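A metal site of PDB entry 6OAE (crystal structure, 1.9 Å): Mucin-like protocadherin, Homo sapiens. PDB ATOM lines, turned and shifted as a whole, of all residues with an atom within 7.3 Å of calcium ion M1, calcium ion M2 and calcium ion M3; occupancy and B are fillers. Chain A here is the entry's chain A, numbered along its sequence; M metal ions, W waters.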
ATOM      1  N   GLU A  17      12.077 -25.024   5.558  1.00  0.00           N
ATOM      2  CA  GLU A  17      13.067 -26.057   5.171  1.00  0.00           C
ATOM      3  C   GLU A  17      12.414 -27.419   5.314  1.00  0.00           C
ATOM      4  O   GLU A  17      11.461 -27.552   6.121  1.00  0.00           O
ATOM      5  CB  GLU A  17      14.347 -25.943   5.988  1.00  0.00           C
ATOM      6  CG  GLU A  17      14.143 -26.096   7.487  1.00  0.00           C
ATOM      7  CD  GLU A  17      15.441 -26.348   8.222  1.00  0.00           C
ATOM      8  OE1 GLU A  17      15.490 -26.027   9.418  1.00  0.00           O
ATOM      9  OE2 GLU A  17      16.376 -26.862   7.597  1.00  0.00           O
ATOM     10  N   ASN A  18      12.888 -28.390   4.529  1.00  0.00           N
ATOM     11  CA  ASN A  18      12.398 -29.796   4.497  1.00  0.00           C
ATOM     12  C   ASN A  18      11.019 -29.878   3.828  1.00  0.00           C
ATOM     13  O   ASN A  18      10.465 -30.959   3.843  1.00  0.00           O
ATOM     14  CB  ASN A  18      12.429 -30.437   5.891  1.00  0.00           C
ATOM     15  CG  ASN A  18      13.797 -30.284   6.528  1.00  0.00           C
ATOM     16  OD1 ASN A  18      14.804 -30.327   5.829  1.00  0.00           O
ATOM     17  ND2 ASN A  18      13.834 -30.108   7.835  1.00  0.00           N
ATOM     18  N   PRO A  60      14.717 -27.500   0.450  1.00  0.00           N
ATOM     19  CA  PRO A  60      15.689 -26.625   1.091  1.00  0.00           C
ATOM     20  C   PRO A  60      16.109 -27.087   2.489  1.00  0.00           C
ATOM     21  O   PRO A  60      15.347 -27.815   3.146  1.00  0.00           O
ATOM     22  CB  PRO A  60      14.954 -25.282   1.254  1.00  0.00           C
ATOM     23  CG  PRO A  60      13.780 -25.371   0.334  1.00  0.00           C
ATOM     24  CD  PRO A  60      13.427 -26.831   0.254  1.00  0.00           C
ATOM     25  N   ASP A  61      17.304 -26.669   2.893  1.00  0.00           N
ATOM     26  CA  ASP A  61      17.895 -26.943   4.221  1.00  0.00           C
ATOM     27  C   ASP A  61      18.475 -25.640   4.739  1.00  0.00           C
ATOM     28  O   ASP A  61      19.509 -25.206   4.226  1.00  0.00           O
ATOM     29  CB  ASP A  61      18.941 -28.047   4.142  1.00  0.00           C
ATOM     30  CG  ASP A  61      19.715 -28.278   5.438  1.00  0.00           C
ATOM     31  OD1 ASP A  61      19.319 -27.719   6.460  1.00  0.00           O
ATOM     32  OD2 ASP A  61      20.714 -28.989   5.388  1.00  0.00           O
ATOM     33  N   TYR A  62      17.815 -25.053   5.732  1.00  0.00           N
ATOM     34  CA  TYR A  62      18.199 -23.764   6.359  1.00  0.00           C
ATOM     35  C   TYR A  62      19.662 -23.779   6.837  1.00  0.00           C
ATOM     36  O   TYR A  62      20.326 -22.711   6.765  1.00  0.00           O
ATOM     37  CB  TYR A  62      17.259 -23.432   7.498  1.00  0.00           C
ATOM     38  CG  TYR A  62      17.522 -22.094   8.108  1.00  0.00           C
ATOM     39  CD1 TYR A  62      16.922 -20.952   7.609  1.00  0.00           C
ATOM     40  CD2 TYR A  62      18.399 -21.953   9.178  1.00  0.00           C
ATOM     41  CE1 TYR A  62      17.165 -19.693   8.157  1.00  0.00           C
ATOM     42  CE2 TYR A  62      18.653 -20.708   9.739  1.00  0.00           C
ATOM     43  CZ  TYR A  62      18.038 -19.577   9.216  1.00  0.00           C
ATOM     44  OH  TYR A  62      18.292 -18.357   9.778  1.00  0.00           O
ATOM     45  N   GLU A  63      20.170 -24.934   7.291  1.00  0.00           N
ATOM     46  CA  GLU A  63      21.568 -25.085   7.793  1.00  0.00           C
ATOM     47  C   GLU A  63      22.581 -25.106   6.621  1.00  0.00           C
ATOM     48  O   GLU A  63      23.750 -24.838   6.866  1.00  0.00           O
ATOM     49  CB  GLU A  63      21.671 -26.336   8.667  1.00  0.00           C
ATOM     50  CG  GLU A  63      21.097 -26.165  10.074  1.00  0.00           C
ATOM     51  CD  GLU A  63      19.578 -26.065  10.196  1.00  0.00           C
ATOM     52  OE1 GLU A  63      18.877 -26.976   9.701  1.00  0.00           O
ATOM     53  OE2 GLU A  63      19.085 -25.106  10.808  1.00  0.00           O
ATOM     54  N   GLU A  64      22.153 -25.422   5.397  1.00  0.00           N
ATOM     55  CA  GLU A  64      23.036 -25.428   4.199  1.00  0.00           C
ATOM     56  C   GLU A  64      22.953 -24.066   3.503  1.00  0.00           C
ATOM     57  O   GLU A  64      24.023 -23.498   3.199  1.00  0.00           O
ATOM     58  CB  GLU A  64      22.636 -26.621   3.317  1.00  0.00           C
ATOM     59  CG  GLU A  64      23.442 -26.762   2.027  1.00  0.00           C
ATOM     60  CD  GLU A  64      22.783 -26.214   0.774  1.00  0.00           C
ATOM     61  OE1 GLU A  64      21.530 -26.266   0.666  1.00  0.00           O
ATOM     62  OE2 GLU A  64      23.526 -25.736  -0.118  1.00  0.00           O
ATOM     63  N   LEU A  91      12.856 -20.825   5.731  1.00  0.00           N
ATOM     64  CA  LEU A  91      12.526 -20.621   7.161  1.00  0.00           C
ATOM     65  C   LEU A  91      13.091 -21.788   7.963  1.00  0.00           C
ATOM     66  O   LEU A  91      12.909 -22.963   7.553  1.00  0.00           O
ATOM     67  CB  LEU A  91      11.014 -20.528   7.363  1.00  0.00           C
ATOM     68  CG  LEU A  91      10.299 -19.434   6.563  1.00  0.00           C
ATOM     69  CD1 LEU A  91       8.812 -19.424   6.919  1.00  0.00           C
ATOM     70  CD2 LEU A  91      10.927 -18.072   6.800  1.00  0.00           C
ATOM     71  N   ASP A  92      13.734 -21.463   9.065  1.00  0.00           N
ATOM     72  CA  ASP A  92      14.335 -22.466   9.962  1.00  0.00           C
ATOM     73  C   ASP A  92      13.226 -23.254  10.653  1.00  0.00           C
ATOM     74  O   ASP A  92      12.181 -22.667  11.069  1.00  0.00           O
ATOM     75  CB  ASP A  92      15.283 -21.824  10.978  1.00  0.00           C
ATOM     76  CG  ASP A  92      15.930 -22.854  11.885  1.00  0.00           C
ATOM     77  OD1 ASP A  92      16.310 -23.961  11.357  1.00  0.00           O
ATOM     78  OD2 ASP A  92      16.007 -22.592  13.113  1.00  0.00           O
ATOM     79  N   VAL A  93      13.444 -24.556  10.750  1.00  0.00           N
ATOM     80  CA  VAL A  93      12.621 -25.537  11.499  1.00  0.00           C
ATOM     81  C   VAL A  93      13.544 -26.135  12.574  1.00  0.00           C
ATOM     82  O   VAL A  93      14.783 -26.234  12.333  1.00  0.00           O
ATOM     83  CB  VAL A  93      12.065 -26.604  10.530  1.00  0.00           C
ATOM     84  CG1 VAL A  93      11.531 -27.842  11.250  1.00  0.00           C
ATOM     85  CG2 VAL A  93      10.999 -26.003   9.612  1.00  0.00           C
ATOM     86  N   ASN A  94      12.979 -26.497  13.721  1.00  0.00           N
ATOM     87  CA  ASN A  94      13.728 -27.220  14.780  1.00  0.00           C
ATOM     88  C   ASN A  94      13.869 -28.674  14.295  1.00  0.00           C
ATOM     89  O   ASN A  94      13.032 -29.516  14.680  1.00  0.00           O
ATOM     90  CB  ASN A  94      13.052 -27.065  16.153  1.00  0.00           C
ATOM     91  CG  ASN A  94      13.801 -27.790  17.249  1.00  0.00           C
ATOM     92  OD1 ASN A  94      14.921 -28.227  17.013  1.00  0.00           O
ATOM     93  ND2 ASN A  94      13.208 -27.917  18.424  1.00  0.00           N
ATOM     94  N   ASP A  95      14.867 -28.947  13.453  1.00  0.00           N
ATOM     95  CA  ASP A  95      15.040 -30.266  12.784  1.00  0.00           C
ATOM     96  C   ASP A  95      16.325 -30.972  13.230  1.00  0.00           C
ATOM     97  O   ASP A  95      16.619 -32.054  12.676  1.00  0.00           O
ATOM     98  CB  ASP A  95      14.949 -30.127  11.254  1.00  0.00           C
ATOM     99  CG  ASP A  95      16.011 -29.266  10.587  1.00  0.00           C
ATOM    100  OD1 ASP A  95      16.579 -28.391  11.253  1.00  0.00           O
ATOM    101  OD2 ASP A  95      16.262 -29.475   9.346  1.00  0.00           O
ATOM    102  N   ASN A  96      17.065 -30.403  14.200  1.00  0.00           N
ATOM    103  CA  ASN A  96      18.331 -30.960  14.738  1.00  0.00           C
ATOM    104  C   ASN A  96      18.182 -31.130  16.258  1.00  0.00           C
ATOM    105  O   ASN A  96      17.543 -30.275  16.903  1.00  0.00           O
ATOM    106  CB  ASN A  96      19.522 -30.070  14.378  1.00  0.00           C
ATOM    107  CG  ASN A  96      19.814 -30.107  12.887  1.00  0.00           C
ATOM    108  OD1 ASN A  96      20.495 -31.014  12.411  1.00  0.00           O
ATOM    109  ND2 ASN A  96      19.301 -29.151  12.152  1.00  0.00           N
ATOM    110  N   ALA A  97      18.737 -32.222  16.782  1.00  0.00           N
ATOM    111  CA  ALA A  97      18.726 -32.523  18.238  1.00  0.00           C
ATOM    112  C   ALA A  97      20.011 -31.969  18.849  1.00  0.00           C
ATOM    113  O   ALA A  97      21.066 -31.934  18.188  1.00  0.00           O
ATOM    114  CB  ALA A  97      18.580 -34.006  18.466  1.00  0.00           C
ATOM    115  N   PRO A  98      19.980 -31.483  20.102  1.00  0.00           N
ATOM    116  CA  PRO A  98      21.209 -31.094  20.780  1.00  0.00           C
ATOM    117  C   PRO A  98      21.982 -32.380  21.077  1.00  0.00           C
ATOM    118  O   PRO A  98      21.381 -33.418  21.268  1.00  0.00           O
ATOM    119  CB  PRO A  98      20.743 -30.336  22.040  1.00  0.00           C
ATOM    120  CG  PRO A  98      19.351 -30.902  22.306  1.00  0.00           C
ATOM    121  CD  PRO A  98      18.794 -31.260  20.941  1.00  0.00           C
ATOM    122  N   ASP A 129      23.755 -27.746  19.097  1.00  0.00           N
ATOM    123  CA  ASP A 129      22.557 -28.001  18.271  1.00  0.00           C
ATOM    124  C   ASP A 129      22.774 -27.297  16.934  1.00  0.00           C
ATOM    125  O   ASP A 129      23.006 -26.058  16.951  1.00  0.00           O
ATOM    126  CB  ASP A 129      21.334 -27.512  19.058  1.00  0.00           C
ATOM    127  CG  ASP A 129      20.017 -27.856  18.426  1.00  0.00           C
ATOM    128  OD1 ASP A 129      19.919 -27.805  17.174  1.00  0.00           O
ATOM    129  OD2 ASP A 129      19.089 -28.163  19.194  1.00  0.00           O
ATOM    130  N   ARG A 130      22.711 -28.038  15.820  1.00  0.00           N
ATOM    131  CA  ARG A 130      22.956 -27.483  14.456  1.00  0.00           C
ATOM    132  C   ARG A 130      21.853 -26.486  14.070  1.00  0.00           C
ATOM    133  O   ARG A 130      22.046 -25.779  13.075  1.00  0.00           O
ATOM    134  CB  ARG A 130      23.150 -28.620  13.439  1.00  0.00           C
ATOM    135  CG  ARG A 130      24.424 -29.432  13.658  1.00  0.00           C
ATOM    136  CD  ARG A 130      24.640 -30.497  12.599  1.00  0.00           C
ATOM    137  NE  ARG A 130      25.894 -31.217  12.796  1.00  0.00           N
ATOM    138  CZ  ARG A 130      27.099 -30.720  12.550  1.00  0.00           C
ATOM    139  NH1 ARG A 130      28.182 -31.454  12.781  1.00  0.00           N
ATOM    140  NH2 ARG A 130      27.241 -29.493  12.061  1.00  0.00           N
ATOM    141  N   ASP A 131      20.746 -26.395  14.798  1.00  0.00           N
ATOM    142  CA  ASP A 131      19.827 -25.232  14.727  1.00  0.00           C
ATOM    143  C   ASP A 131      20.530 -24.109  15.495  1.00  0.00           C
ATOM    144  O   ASP A 131      20.356 -24.025  16.729  1.00  0.00           O
ATOM    145  CB  ASP A 131      18.451 -25.553  15.290  1.00  0.00           C
ATOM    146  CG  ASP A 131      17.774 -26.699  14.582  1.00  0.00           C
ATOM    147  OD1 ASP A 131      17.766 -26.670  13.332  1.00  0.00           O
ATOM    148  OD2 ASP A 131      17.273 -27.615  15.260  1.00  0.00           O
ATOM    149  N   LYS A 132      21.306 -23.289  14.804  1.00  0.00           N
ATOM    150  CA  LYS A 132      22.206 -22.286  15.429  1.00  0.00           C
ATOM    151  C   LYS A 132      21.417 -21.331  16.346  1.00  0.00           C
ATOM    152  O   LYS A 132      22.008 -20.821  17.286  1.00  0.00           O
ATOM    153  CB  LYS A 132      22.908 -21.453  14.358  1.00  0.00           C
ATOM    154  CG  LYS A 132      23.984 -22.160  13.546  1.00  0.00           C
ATOM    155  CD  LYS A 132      24.964 -21.181  12.889  1.00  0.00           C
ATOM    156  CE  LYS A 132      24.491 -20.576  11.572  1.00  0.00           C
ATOM    157  NZ  LYS A 132      23.146 -19.948  11.620  1.00  0.00           N
ATOM    158  N   ASP A 134      18.729 -22.045  18.222  1.00  0.00           N
ATOM    159  CA  ASP A 134      18.060 -22.734  19.360  1.00  0.00           C
ATOM    160  C   ASP A 134      18.791 -22.372  20.662  1.00  0.00           C
ATOM    161  O   ASP A 134      20.022 -22.534  20.697  1.00  0.00           O
ATOM    162  CB  ASP A 134      18.007 -24.251  19.159  1.00  0.00           C
ATOM    163  CG  ASP A 134      16.914 -24.728  18.221  1.00  0.00           C
ATOM    164  OD1 ASP A 134      16.187 -23.864  17.665  1.00  0.00           O
ATOM    165  OD2 ASP A 134      16.770 -25.962  18.078  1.00  0.00           O
ATOM    166  N   LEU A 136      19.479 -23.512  24.378  1.00  0.00           N
ATOM    167  CA  LEU A 136      19.454 -24.844  25.024  1.00  0.00           C
ATOM    168  C   LEU A 136      19.182 -24.670  26.520  1.00  0.00           C
ATOM    169  O   LEU A 136      19.693 -23.727  27.125  1.00  0.00           O
ATOM    170  CB  LEU A 136      20.778 -25.562  24.737  1.00  0.00           C
ATOM    171  CG  LEU A 136      21.059 -25.787  23.250  1.00  0.00           C
ATOM    172  CD1 LEU A 136      22.265 -26.694  23.067  1.00  0.00           C
ATOM    173  CD2 LEU A 136      19.851 -26.352  22.519  1.00  0.00           C
ATOM    174  N   ARG A 182      17.538 -29.785  26.457  1.00  0.00           N
ATOM    175  CA  ARG A 182      16.462 -29.736  25.428  1.00  0.00           C
ATOM    176  C   ARG A 182      16.643 -28.428  24.667  1.00  0.00           C
ATOM    177  O   ARG A 182      17.282 -27.486  25.216  1.00  0.00           O
ATOM    178  CB  ARG A 182      15.073 -29.909  26.050  1.00  0.00           C
ATOM    179  CG  ARG A 182      14.678 -28.825  27.024  1.00  0.00           C
ATOM    180  CD  ARG A 182      13.219 -28.827  27.484  1.00  0.00           C
ATOM    181  NE  ARG A 182      12.996 -27.638  28.314  1.00  0.00           N
ATOM    182  CZ  ARG A 182      13.254 -27.529  29.630  1.00  0.00           C
ATOM    183  NH1 ARG A 182      13.720 -28.549  30.333  1.00  0.00           N
ATOM    184  NH2 ARG A 182      13.014 -26.392  30.237  1.00  0.00           N
ATOM    185  N   ASP A 183      16.093 -28.358  23.445  1.00  0.00           N
ATOM    186  CA  ASP A 183      16.251 -27.183  22.552  1.00  0.00           C
ATOM    187  C   ASP A 183      14.975 -26.332  22.553  1.00  0.00           C
ATOM    188  O   ASP A 183      14.819 -25.535  21.641  1.00  0.00           O
ATOM    189  CB  ASP A 183      16.654 -27.633  21.155  1.00  0.00           C
ATOM    190  CG  ASP A 183      15.717 -28.636  20.490  1.00  0.00           C
ATOM    191  OD1 ASP A 183      14.630 -28.943  21.070  1.00  0.00           O
ATOM    192  OD2 ASP A 183      16.112 -29.113  19.410  1.00  0.00           O
ATOM    193  N   THR A 184      14.092 -26.496  23.541  1.00  0.00           N
ATOM    194  CA  THR A 184      12.845 -25.702  23.709  1.00  0.00           C
ATOM    195  C   THR A 184      12.694 -25.311  25.172  1.00  0.00           C
ATOM    196  O   THR A 184      13.089 -26.058  26.070  1.00  0.00           O
ATOM    197  CB  THR A 184      11.619 -26.479  23.223  1.00  0.00           C
ATOM    198  OG1 THR A 184      11.455 -27.665  24.022  1.00  0.00           O
ATOM    199  CG2 THR A 184      11.724 -26.819  21.749  1.00  0.00           C
ATOM    200  N   SER A 192      10.479 -30.930  19.917  1.00  0.00           N
ATOM    201  CA  SER A 192      11.467 -30.732  21.015  1.00  0.00           C
ATOM    202  C   SER A 192      12.416 -31.937  21.049  1.00  0.00           C
ATOM    203  O   SER A 192      11.926 -33.052  20.964  1.00  0.00           O
ATOM    204  CB  SER A 192      10.793 -30.531  22.340  1.00  0.00           C
ATOM    205  OG  SER A 192      11.760 -30.306  23.353  1.00  0.00           O
ATOM    206  N   HIS A 193      13.707 -31.706  21.183  1.00  0.00           N
ATOM    207  CA  HIS A 193      14.711 -32.793  21.198  1.00  0.00           C
ATOM    208  C   HIS A 193      15.469 -32.728  22.506  1.00  0.00           C
ATOM    209  O   HIS A 193      15.792 -31.607  22.920  1.00  0.00           O
ATOM    210  CB  HIS A 193      15.655 -32.660  20.022  1.00  0.00           C
ATOM    211  CG  HIS A 193      14.956 -32.506  18.715  1.00  0.00           C
ATOM    212  ND1 HIS A 193      14.852 -31.290  18.104  1.00  0.00           N
ATOM    213  CD2 HIS A 193      14.318 -33.408  17.924  1.00  0.00           C
ATOM    214  CE1 HIS A 193      14.190 -31.430  16.965  1.00  0.00           C
ATOM    215  NE2 HIS A 193      13.835 -32.729  16.843  1.00  0.00           N
HETATM  216 CA    CA M   1      17.923 -28.513   8.241  1.00  0.00          CA
HETATM  217 CA    CA M   2      16.892 -26.120  11.292  1.00  0.00          CA
HETATM  218 CA    CA M   3      17.205 -28.127  17.614  1.00  0.00          CA
HETATM  219  O   HOH W   1      17.380 -30.118   6.528  1.00  0.00           O
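The side-chain carboxylate of Asp 183 is in hydrogen-bond range of the backbone NH of His 193 (2.9 Å).
OD1 of Asn 94 lies close to ND1 of His 193.
The side-chain carboxylate of Asp 95 sits close to the side-chain amide nitrogen of Asn 18 (2.9 Å).
The backbone NH (N) of Glu 17 is in hydrogen-bond range of the backbone carbonyl oxygen (O) of Leu 91 (3.0 Å).
The backbone carbonyl oxygen (O) of Asn 96 sits close to a ring nitrogen (ND1) of His 193, at 3.1 Å.
The side-chain carboxylate (OE2) of Glu 17 lies close to the backbone NH (N) of Tyr 62, 3.0 Å away.
The side-chain amide nitrogen (ND2) of Asn 96 lies close to the side-chain carboxylate (OE1) of Glu 63 (3.3 Å).
The side-chain carboxylate of Asp 95 sits close to the side-chain amide nitrogen of Asn 96, 3.0 Å away.
The nearest printed residue that does not touch calcium ion M2 is Asn 94 (4.6 Å).
His 193 touches calcium ion M3 (ND1 to CA, 3.97 Å).
Seven residues have an atom within 4 Å of calcium ion M3: Asn 94, Asn 96, Asp 129, Asp 131, Asp 134, Asp 183 and His 193.
The nearest printed residue that does not touch calcium ion M3 is Ala 97 (4.5 Å).
Calcium ion M1 is bound by OD2 of Asp 95 (2.2 Å), OE1 of Glu 63 (2.3 Å), OE2 of Glu 17 (2.4 Å), OD1 of Asp 61 (2.4 Å) and water W1 (2.4 Å).
Calcium ion M1 has five donor atoms within binding distance.
Calcium ion M2 is bound by the side-chain carboxylate (OD1) of Asp 92 (2.2 Å), the side-chain carboxylate (OD1) of Asp 131 (2.3 Å), the side-chain carboxylate (OD1) of Asp 95 (2.3 Å), the side-chain carboxylate (OE1) of Glu 17 (2.3 Å), the backbone carbonyl oxygen (O) of Val 93 (2.4 Å), the side-chain carboxylate (OE2) of Glu 63 (2.5 Å) and the side-chain carboxylate (OE1) of Glu 63 (2.7 Å).
Calcium ion M3 is bound by the side-chain carboxylate (OD2) of Asp 134 (2.3 Å), the backbone carbonyl oxygen (O) of Asn 96 (2.3 Å), the side-chain carboxylate (OD2) of Asp 183 (2.3 Å), the side-chain amide oxygen (OD1) of Asn 94 (2.4 Å), the side-chain carboxylate (OD2) of Asp 131 (2.4 Å), the side-chain carboxylate (OD2) of Asp 129 (2.5 Å) and the side-chain carboxylate (OD1) of Asp 129 (2.8 Å).
Calcium ion M3 has seven donor atoms within binding distance.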
